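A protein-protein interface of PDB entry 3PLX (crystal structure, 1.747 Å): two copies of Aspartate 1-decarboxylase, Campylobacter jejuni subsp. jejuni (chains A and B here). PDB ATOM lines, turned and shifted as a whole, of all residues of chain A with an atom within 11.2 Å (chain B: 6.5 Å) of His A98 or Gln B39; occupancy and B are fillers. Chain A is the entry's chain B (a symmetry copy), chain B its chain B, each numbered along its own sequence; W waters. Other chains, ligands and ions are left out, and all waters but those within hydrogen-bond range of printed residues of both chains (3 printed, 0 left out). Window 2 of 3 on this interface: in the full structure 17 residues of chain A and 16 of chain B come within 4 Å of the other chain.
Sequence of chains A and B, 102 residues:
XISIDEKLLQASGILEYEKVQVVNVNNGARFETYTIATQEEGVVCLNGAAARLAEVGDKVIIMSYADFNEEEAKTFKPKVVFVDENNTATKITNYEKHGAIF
OE1 of Glu B16 sits at hydrogen-bond distance from N of His A98 (3.0 Å).
The side-chain hydroxyl of Tyr B17 sits at hydrogen-bond distance from the backbone NH of Gly A99 (3.2 Å).
A ring nitrogen (NE2) of His A98 sits at hydrogen-bond distance from the side-chain carboxylate of Glu B6 (2.6 Å).
OH of Tyr B17 sits at hydrogen-bond distance from O of Glu A96 (2.5 Å).
OE2 of Glu B16 lies within hydrogen-bond range of N of Gly A99, at 2.9 Å.
O of Ile B36 lies within hydrogen-bond range of N of Ile B4 (2.9 Å).
N of Ala B37 lies within hydrogen-bond range of OE2 of Glu B16 (2.7 Å).
ND2 of Asn A94 sits close to O of Pro A78 (3.4 Å).
The backbone NH (N) of Tyr A95 is in hydrogen-bond range of the backbone carbonyl oxygen (O) of Pro A78, 3.0 Å away.
The backbone NH of Glu B6 is in hydrogen-bond range of the backbone carbonyl oxygen of Thr B38, 2.9 Å away.
The side-chain hydroxyl (OH) of Tyr B17 lies within hydrogen-bond range of the side-chain carboxylate (OE2) of Glu B16.
Among the printed residues, merely in contact across the chains: Pro A78 with Tyr B17, Tyr A95 with Tyr B17, Lys A97 with Glu B16, His A98 with Ala B37, His A98 with Gln B39 and Gly A99 with Ile B36.
Of chain B, only Glu B6 (2.6 Å), Glu B16 (3.0 Å), Ala B37 (3.1 Å) and Gln B39 (3.3 Å) come within 4 Å of His A98.
Of the printed residues of chain A, Gln B39 touches His A98.
Ala B37 touches one residue of chain A.
No residue of chain A comes within 4 Å of Thr B38.
Of the printed residues of chain A, Glu B6 touches His A98 (2.6 Å).
Of the printed residues of chain B, Gly A99 touches Glu B16, Tyr B17 and Ile B36.
Of the printed residues of chain A, Tyr B17 touches Pro A78, Tyr A95, Glu A96 and Gly A99.
Of the printed residues of chain A, Ile B36 touches Gly A99.
Printed residues of chain B within 4 Å of Tyr A95: Tyr B17 (3.2 Å).
The nearest residue of chain A that does not touch Gln B39 is Lys A97 (6.7 Å).
The nearest printed residue of chain A that does not touch Glu B6 is Lys A97 (4.9 Å).
Of the 13 printed residues of chain A, 6 touch a printed residue of chain B.
Hydrophobic or aromatic side chains of chain A within 4 Å of the printed part of chain B: Pro A78, Tyr A95 and His A98.
Along chain A the printed residues that touch a printed residue of chain B span positions 78 to 99.
Among the printed residues, 11 pairs touch across the chains.
No position is printed for both chains.
Of the 11 pairs that touch across the chains among the printed residues, none has its exchanged pair printed and touching as well.
Water W3 bridges OE1 of Glu B16 (2.7 Å) and NZ of Lys A77 (2.8 Å).
Water W1 lies within hydrogen-bond range of O of Ala B37 (2.7 Å) and O of His A98 (2.9 Å).
Water W2 lies within hydrogen-bond range of the side-chain amino group of Lys A97 (3.0 Å) and the side-chain carboxylate of Glu B16 (3.0 Å).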
ATOM      1  N   LYS A  74      -5.283 -22.639  18.174  1.00  0.00           N
ATOM      2  CA  LYS A  74      -6.007 -21.415  18.495  1.00  0.00           C
ATOM      3  C   LYS A  74      -7.156 -21.646  19.473  1.00  0.00           C
ATOM      4  O   LYS A  74      -7.443 -20.792  20.310  1.00  0.00           O
ATOM      5  CB  LYS A  74      -6.557 -20.768  17.219  1.00  0.00           C
ATOM      6  CG  LYS A  74      -5.525 -20.050  16.366  1.00  0.00           C
ATOM      7  CD  LYS A  74      -6.183 -19.444  15.132  1.00  0.00           C
ATOM      8  CE  LYS A  74      -5.239 -18.524  14.369  1.00  0.00           C
ATOM      9  NZ  LYS A  74      -4.072 -19.251  13.802  1.00  0.00           N
ATOM     10  N   PHE A  76      -7.712 -24.661  21.386  1.00  0.00           N
ATOM     11  CA  PHE A  76      -7.514 -25.699  22.394  1.00  0.00           C
ATOM     12  C   PHE A  76      -7.499 -25.129  23.810  1.00  0.00           C
ATOM     13  O   PHE A  76      -6.871 -24.103  24.071  1.00  0.00           O
ATOM     14  CB  PHE A  76      -6.216 -26.474  22.132  1.00  0.00           C
ATOM     15  CG  PHE A  76      -5.966 -27.575  23.118  1.00  0.00           C
ATOM     16  CD1 PHE A  76      -6.637 -28.783  23.008  1.00  0.00           C
ATOM     17  CD2 PHE A  76      -5.065 -27.400  24.169  1.00  0.00           C
ATOM     18  CE1 PHE A  76      -6.419 -29.799  23.924  1.00  0.00           C
ATOM     19  CE2 PHE A  76      -4.844 -28.403  25.082  1.00  0.00           C
ATOM     20  CZ  PHE A  76      -5.516 -29.611  24.962  1.00  0.00           C
ATOM     21  N   LYS A  77      -8.187 -25.806  24.727  1.00  0.00           N
ATOM     22  CA  LYS A  77      -8.174 -25.408  26.132  1.00  0.00           C
ATOM     23  C   LYS A  77      -7.614 -26.546  26.980  1.00  0.00           C
ATOM     24  O   LYS A  77      -8.183 -27.637  27.008  1.00  0.00           O
ATOM     25  CB  LYS A  77      -9.578 -25.025  26.614  1.00  0.00           C
ATOM     26  CG  LYS A  77     -10.212 -23.842  25.864  1.00  0.00           C
ATOM     27  CD  LYS A  77      -9.354 -22.583  26.000  1.00  0.00           C
ATOM     28  CE  LYS A  77     -10.006 -21.382  25.319  1.00  0.00           C
ATOM     29  NZ  LYS A  77      -9.184 -20.145  25.459  1.00  0.00           N
ATOM     30  N   PRO A  78      -6.480 -26.305  27.662  1.00  0.00           N
ATOM     31  CA  PRO A  78      -5.893 -27.364  28.487  1.00  0.00           C
ATOM     32  C   PRO A  78      -6.785 -27.777  29.659  1.00  0.00           C
ATOM     33  O   PRO A  78      -7.575 -26.974  30.165  1.00  0.00           O
ATOM     34  CB  PRO A  78      -4.604 -26.721  29.030  1.00  0.00           C
ATOM     35  CG  PRO A  78      -4.283 -25.618  28.063  1.00  0.00           C
ATOM     36  CD  PRO A  78      -5.626 -25.105  27.603  1.00  0.00           C
ATOM     37  N   VAL A  80      -7.243 -28.841  33.540  1.00  0.00           N
ATOM     38  CA  VAL A  80      -6.557 -28.598  34.805  1.00  0.00           C
ATOM     39  C   VAL A  80      -7.261 -29.315  35.946  1.00  0.00           C
ATOM     40  O   VAL A  80      -8.483 -29.224  36.074  1.00  0.00           O
ATOM     41  CB  VAL A  80      -6.494 -27.103  35.148  1.00  0.00           C
ATOM     42  CG1 VAL A  80      -5.685 -26.897  36.427  1.00  0.00           C
ATOM     43  CG2 VAL A  80      -5.867 -26.330  33.999  1.00  0.00           C
ATOM     44  N   ASN A  94     -11.304 -26.705  32.449  1.00  0.00           N
ATOM     45  CA  ASN A  94     -10.417 -26.313  31.375  1.00  0.00           C
ATOM     46  C   ASN A  94     -10.109 -24.836  31.513  1.00  0.00           C
ATOM     47  O   ASN A  94     -10.955 -24.051  31.946  1.00  0.00           O
ATOM     48  CB  ASN A  94     -11.042 -26.604  30.016  1.00  0.00           C
ATOM     49  CG  ASN A  94     -11.221 -28.088  29.774  1.00  0.00           C
ATOM     50  OD1 ASN A  94     -12.151 -28.705  30.293  1.00  0.00           O
ATOM     51  ND2 ASN A  94     -10.328 -28.670  28.992  1.00  0.00           N
ATOM     52  N   TYR A  95      -8.884 -24.472  31.166  1.00  0.00           N
ATOM     53  CA  TYR A  95      -8.481 -23.078  31.143  1.00  0.00           C
ATOM     54  C   TYR A  95      -9.353 -22.287  30.182  1.00  0.00           C
ATOM     55  O   TYR A  95      -9.660 -22.750  29.083  1.00  0.00           O
ATOM     56  CB  TYR A  95      -7.045 -22.969  30.651  1.00  0.00           C
ATOM     57  CG  TYR A  95      -5.984 -22.927  31.719  1.00  0.00           C
ATOM     58  CD1 TYR A  95      -4.890 -23.776  31.656  1.00  0.00           C
ATOM     59  CD2 TYR A  95      -6.050 -22.014  32.766  1.00  0.00           C
ATOM     60  CE1 TYR A  95      -3.893 -23.736  32.606  1.00  0.00           C
ATOM     61  CE2 TYR A  95      -5.049 -21.966  33.733  1.00  0.00           C
ATOM     62  CZ  TYR A  95      -3.972 -22.832  33.642  1.00  0.00           C
ATOM     63  OH  TYR A  95      -2.967 -22.799  34.580  1.00  0.00           O
ATOM     64  N   GLU A  96      -9.744 -21.087  30.592  1.00  0.00           N
ATOM     65  CA  GLU A  96     -10.368 -20.145  29.672  1.00  0.00           C
ATOM     66  C   GLU A  96      -9.355 -19.047  29.369  1.00  0.00           C
ATOM     67  O   GLU A  96      -8.223 -19.094  29.850  1.00  0.00           O
ATOM     68  CB  GLU A  96     -11.652 -19.561  30.267  1.00  0.00           C
ATOM     69  CG  GLU A  96     -12.766 -20.584  30.448  1.00  0.00           C
ATOM     70  CD  GLU A  96     -13.125 -21.292  29.151  1.00  0.00           C
ATOM     71  OE1 GLU A  96     -13.023 -20.661  28.075  1.00  0.00           O
ATOM     72  OE2 GLU A  96     -13.509 -22.480  29.206  1.00  0.00           O
ATOM     73  N   LYS A  97      -9.758 -18.061  28.574  1.00  0.00           N
ATOM     74  CA  LYS A  97      -8.856 -16.977  28.206  1.00  0.00           C
ATOM     75  C   LYS A  97      -8.298 -16.281  29.454  1.00  0.00           C
ATOM     76  O   LYS A  97      -8.986 -16.165  30.477  1.00  0.00           O
ATOM     77  CB  LYS A  97      -9.585 -15.982  27.304  1.00  0.00           C
ATOM     78  CG  LYS A  97      -8.673 -15.098  26.467  1.00  0.00           C
ATOM     79  CD  LYS A  97      -9.492 -14.232  25.516  1.00  0.00           C
ATOM     80  CE  LYS A  97      -8.605 -13.331  24.669  1.00  0.00           C
ATOM     81  NZ  LYS A  97      -7.676 -14.110  23.799  1.00  0.00           N
ATOM     82  N   HIS A  98      -7.048 -15.832  29.369  1.00  0.00           N
ATOM     83  CA  HIS A  98      -6.388 -15.122  30.470  1.00  0.00           C
ATOM     84  C   HIS A  98      -6.261 -15.943  31.754  1.00  0.00           C
ATOM     85  O   HIS A  98      -6.434 -15.413  32.854  1.00  0.00           O
ATOM     86  CB  HIS A  98      -7.091 -13.797  30.775  1.00  0.00           C
ATOM     87  CG  HIS A  98      -7.163 -12.873  29.602  1.00  0.00           C
ATOM     88  ND1 HIS A  98      -8.355 -12.476  29.037  1.00  0.00           N
ATOM     89  CD2 HIS A  98      -6.184 -12.281  28.874  1.00  0.00           C
ATOM     90  CE1 HIS A  98      -8.110 -11.669  28.018  1.00  0.00           C
ATOM     91  NE2 HIS A  98      -6.800 -11.536  27.900  1.00  0.00           N
ATOM     92  N   GLY A  99      -5.955 -17.228  31.613  1.00  0.00           N
ATOM     93  CA  GLY A  99      -5.736 -18.091  32.762  1.00  0.00           C
ATOM     94  C   GLY A  99      -6.941 -18.277  33.670  1.00  0.00           C
ATOM     95  O   GLY A  99      -6.803 -18.763  34.793  1.00  0.00           O
ATOM     96  N   ALA A 100      -8.121 -17.895  33.193  1.00  0.00           N
ATOM     97  CA  ALA A 100      -9.344 -18.053  33.981  1.00  0.00           C
ATOM     98  C   ALA A 100      -9.687 -19.531  34.232  1.00  0.00           C
ATOM     99  O   ALA A 100      -9.553 -20.373  33.342  1.00  0.00           O
ATOM    100  CB  ALA A 100     -10.515 -17.324  33.318  1.00  0.00           C
ATOM    101  N   ILE A 101     -10.124 -19.831  35.452  1.00  0.00           N
ATOM    102  CA  ILE A 101     -10.446 -21.199  35.851  1.00  0.00           C
ATOM    103  C   ILE A 101     -11.880 -21.317  36.364  1.00  0.00           C
ATOM    104  O   ILE A 101     -12.297 -20.569  37.251  1.00  0.00           O
ATOM    105  CB  ILE A 101      -9.470 -21.708  36.933  1.00  0.00           C
ATOM    106  CG1 ILE A 101      -8.095 -21.981  36.322  1.00  0.00           C
ATOM    107  CG2 ILE A 101     -10.006 -22.967  37.590  1.00  0.00           C
ATOM    108  CD1 ILE A 101      -8.107 -23.075  35.276  1.00  0.00           C
ATOM    109  N   ILE B   4       2.070 -13.412  31.127  1.00  0.00           N
ATOM    110  CA  ILE B   4       2.686 -12.415  30.276  1.00  0.00           C
ATOM    111  C   ILE B   4       1.607 -11.517  29.691  1.00  0.00           C
ATOM    112  O   ILE B   4       0.570 -11.996  29.247  1.00  0.00           O
ATOM    113  CB  ILE B   4       3.460 -13.083  29.119  1.00  0.00           C
ATOM    114  CG1 ILE B   4       4.573 -13.982  29.666  1.00  0.00           C
ATOM    115  CG2 ILE B   4       4.020 -12.026  28.169  1.00  0.00           C
ATOM    116  CD1 ILE B   4       5.169 -14.879  28.606  1.00  0.00           C
ATOM    117  N   ASP B   5       1.860 -10.215  29.728  1.00  0.00           N
ATOM    118  CA  ASP B   5       1.012  -9.222  29.078  1.00  0.00           C
ATOM    119  C   ASP B   5       0.559  -9.748  27.717  1.00  0.00           C
ATOM    120  O   ASP B   5       1.385 -10.095  26.877  1.00  0.00           O
ATOM    121  CB  ASP B   5       1.832  -7.943  28.905  1.00  0.00           C
ATOM    122  CG  ASP B   5       1.055  -6.812  28.259  1.00  0.00           C
ATOM    123  OD1 ASP B   5      -0.104  -7.010  27.824  1.00  0.00           O
ATOM    124  OD2 ASP B   5       1.620  -5.702  28.210  1.00  0.00           O
ATOM    125  N   GLU B   6      -0.752  -9.810  27.500  1.00  0.00           N
ATOM    126  CA  GLU B   6      -1.281 -10.293  26.230  1.00  0.00           C
ATOM    127  C   GLU B   6      -0.730  -9.505  25.043  1.00  0.00           C
ATOM    128  O   GLU B   6      -0.655 -10.030  23.931  1.00  0.00           O
ATOM    129  CB  GLU B   6      -2.812 -10.244  26.220  1.00  0.00           C
ATOM    130  CG  GLU B   6      -3.385  -8.849  26.360  1.00  0.00           C
ATOM    131  CD  GLU B   6      -4.910  -8.849  26.403  1.00  0.00           C
ATOM    132  OE1 GLU B   6      -5.515  -9.928  26.245  1.00  0.00           O
ATOM    133  OE2 GLU B   6      -5.498  -7.772  26.596  1.00  0.00           O
ATOM    134  N   LYS B   7      -0.342  -8.254  25.273  1.00  0.00           N
ATOM    135  CA  LYS B   7       0.243  -7.445  24.198  1.00  0.00           C
ATOM    136  C   LYS B   7       1.552  -8.070  23.699  1.00  0.00           C
ATOM    137  O   LYS B   7       1.850  -8.049  22.502  1.00  0.00           O
ATOM    138  CB  LYS B   7       0.498  -6.010  24.669  1.00  0.00           C
ATOM    139  CG  LYS B   7      -0.776  -5.172  24.853  1.00  0.00           C
ATOM    140  CD  LYS B   7      -0.454  -3.839  25.540  1.00  0.00           C
ATOM    141  CE  LYS B   7      -1.665  -2.914  25.571  1.00  0.00           C
ATOM    142  NZ  LYS B   7      -2.845  -3.537  26.231  1.00  0.00           N
ATOM    143  N   GLU B  16      -1.403 -18.158  24.133  1.00  0.00           N
ATOM    144  CA  GLU B  16      -1.671 -18.531  25.513  1.00  0.00           C
ATOM    145  C   GLU B  16      -1.653 -20.061  25.615  1.00  0.00           C
ATOM    146  O   GLU B  16      -2.192 -20.754  24.749  1.00  0.00           O
ATOM    147  CB  GLU B  16      -3.025 -17.978  25.976  1.00  0.00           C
ATOM    148  CG  GLU B  16      -3.257 -18.252  27.448  1.00  0.00           C
ATOM    149  CD  GLU B  16      -4.416 -17.481  28.037  1.00  0.00           C
ATOM    150  OE1 GLU B  16      -5.431 -17.270  27.335  1.00  0.00           O
ATOM    151  OE2 GLU B  16      -4.306 -17.096  29.218  1.00  0.00           O
ATOM    152  N   TYR B  17      -1.018 -20.568  26.669  1.00  0.00           N
ATOM    153  CA  TYR B  17      -0.835 -22.009  26.925  1.00  0.00           C
ATOM    154  C   TYR B  17       0.234 -22.670  26.056  1.00  0.00           C
ATOM    155  O   TYR B  17       0.467 -23.873  26.167  1.00  0.00           O
ATOM    156  CB  TYR B  17      -2.162 -22.786  26.911  1.00  0.00           C
ATOM    157  CG  TYR B  17      -3.193 -22.080  27.758  1.00  0.00           C
ATOM    158  CD1 TYR B  17      -2.907 -21.747  29.076  1.00  0.00           C
ATOM    159  CD2 TYR B  17      -4.422 -21.690  27.229  1.00  0.00           C
ATOM    160  CE1 TYR B  17      -3.835 -21.064  29.861  1.00  0.00           C
ATOM    161  CE2 TYR B  17      -5.351 -21.011  28.004  1.00  0.00           C
ATOM    162  CZ  TYR B  17      -5.047 -20.703  29.316  1.00  0.00           C
ATOM    163  OH  TYR B  17      -5.954 -20.029  30.099  1.00  0.00           O
ATOM    164  N   ILE B  36       0.592 -17.966  30.350  1.00  0.00           N
ATOM    165  CA  ILE B  36      -0.761 -17.557  30.693  1.00  0.00           C
ATOM    166  C   ILE B  36      -0.880 -16.094  30.297  1.00  0.00           C
ATOM    167  O   ILE B  36       0.021 -15.318  30.563  1.00  0.00           O
ATOM    168  CB  ILE B  36      -1.010 -17.690  32.204  1.00  0.00           C
ATOM    169  CG1 ILE B  36      -0.879 -19.156  32.627  1.00  0.00           C
ATOM    170  CG2 ILE B  36      -2.399 -17.153  32.559  1.00  0.00           C
ATOM    171  CD1 ILE B  36      -0.792 -19.371  34.140  1.00  0.00           C
ATOM    172  N   ALA B  37      -1.981 -15.716  29.645  1.00  0.00           N
ATOM    173  CA  ALA B  37      -2.159 -14.331  29.245  1.00  0.00           C
ATOM    174  C   ALA B  37      -2.760 -13.499  30.369  1.00  0.00           C
ATOM    175  O   ALA B  37      -3.612 -13.978  31.118  1.00  0.00           O
ATOM    176  CB  ALA B  37      -3.054 -14.244  28.009  1.00  0.00           C
ATOM    177  N   THR B  38      -2.316 -12.252  30.482  1.00  0.00           N
ATOM    178  CA  THR B  38      -2.973 -11.303  31.381  1.00  0.00           C
ATOM    179  C   THR B  38      -3.248 -10.001  30.640  1.00  0.00           C
ATOM    180  O   THR B  38      -2.467  -9.584  29.783  1.00  0.00           O
ATOM    181  CB  THR B  38      -2.127 -11.015  32.644  1.00  0.00           C
ATOM    182  OG1 THR B  38      -2.833 -10.095  33.490  1.00  0.00           O
ATOM    183  CG2 THR B  38      -0.780 -10.416  32.270  1.00  0.00           C
ATOM    184  N   GLN B  39      -4.369  -9.366  30.958  1.00  0.00           N
ATOM    185  CA  GLN B  39      -4.690  -8.082  30.363  1.00  0.00           C
ATOM    186  C   GLN B  39      -3.886  -6.958  31.014  1.00  0.00           C
ATOM    187  O   GLN B  39      -3.841  -5.831  30.503  1.00  0.00           O
ATOM    188  CB  GLN B  39      -6.193  -7.801  30.488  1.00  0.00           C
ATOM    189  CG  GLN B  39      -7.058  -8.813  29.764  1.00  0.00           C
ATOM    190  CD  GLN B  39      -8.537  -8.499  29.868  1.00  0.00           C
ATOM    191  OE1 GLN B  39      -9.153  -8.695  30.916  1.00  0.00           O
ATOM    192  NE2 GLN B  39      -9.118  -8.014  28.777  1.00  0.00           N
ATOM    193  N   GLU B  40      -3.255  -7.259  32.144  1.00  0.00           N
ATOM    194  CA  GLU B  40      -2.509  -6.243  32.872  1.00  0.00           C
ATOM    195  C   GLU B  40      -1.228  -5.893  32.132  1.00  0.00           C
ATOM    196  O   GLU B  40      -0.377  -6.754  31.876  1.00  0.00           O
ATOM    197  CB  GLU B  40      -2.207  -6.686  34.301  1.00  0.00           C
ATOM    198  CG  GLU B  40      -1.582  -5.602  35.148  1.00  0.00           C
ATOM    199  CD  GLU B  40      -1.320  -6.043  36.581  1.00  0.00           C
ATOM    200  OE1 GLU B  40      -1.630  -7.208  36.925  1.00  0.00           O
ATOM    201  OE2 GLU B  40      -0.796  -5.220  37.364  1.00  0.00           O
ATOM    202  N   GLU B  41      -1.093  -4.617  31.796  1.00  0.00           N
ATOM    203  CA  GLU B  41      -0.032  -4.182  30.910  1.00  0.00           C
ATOM    204  C   GLU B  41       1.354  -4.263  31.548  1.00  0.00           C
ATOM    205  O   GLU B  41       1.545  -3.856  32.696  1.00  0.00           O
ATOM    206  CB  GLU B  41      -0.319  -2.756  30.430  1.00  0.00           C
ATOM    207  CG  GLU B  41       0.548  -2.345  29.275  1.00  0.00           C
ATOM    208  CD  GLU B  41       0.019  -1.135  28.537  1.00  0.00           C
ATOM    209  OE1 GLU B  41      -1.139  -0.720  28.787  1.00  0.00           O
ATOM    210  OE2 GLU B  41       0.775  -0.603  27.697  1.00  0.00           O
ATOM    211  N   GLY B  42       2.315  -4.797  30.802  1.00  0.00           N
ATOM    212  CA  GLY B  42       3.701  -4.814  31.241  1.00  0.00           C
ATOM    213  C   GLY B  42       4.094  -5.977  32.139  1.00  0.00           C
ATOM    214  O   GLY B  42       5.256  -6.094  32.536  1.00  0.00           O
HETATM  215  O   HOH W   1      -4.187 -13.918  33.786  1.00  0.00           O
HETATM  216  O   HOH W   2      -5.328 -15.182  25.228  1.00  0.00           O
HETATM  217  O   HOH W   3      -6.696 -18.760  25.439  1.00  0.00           O
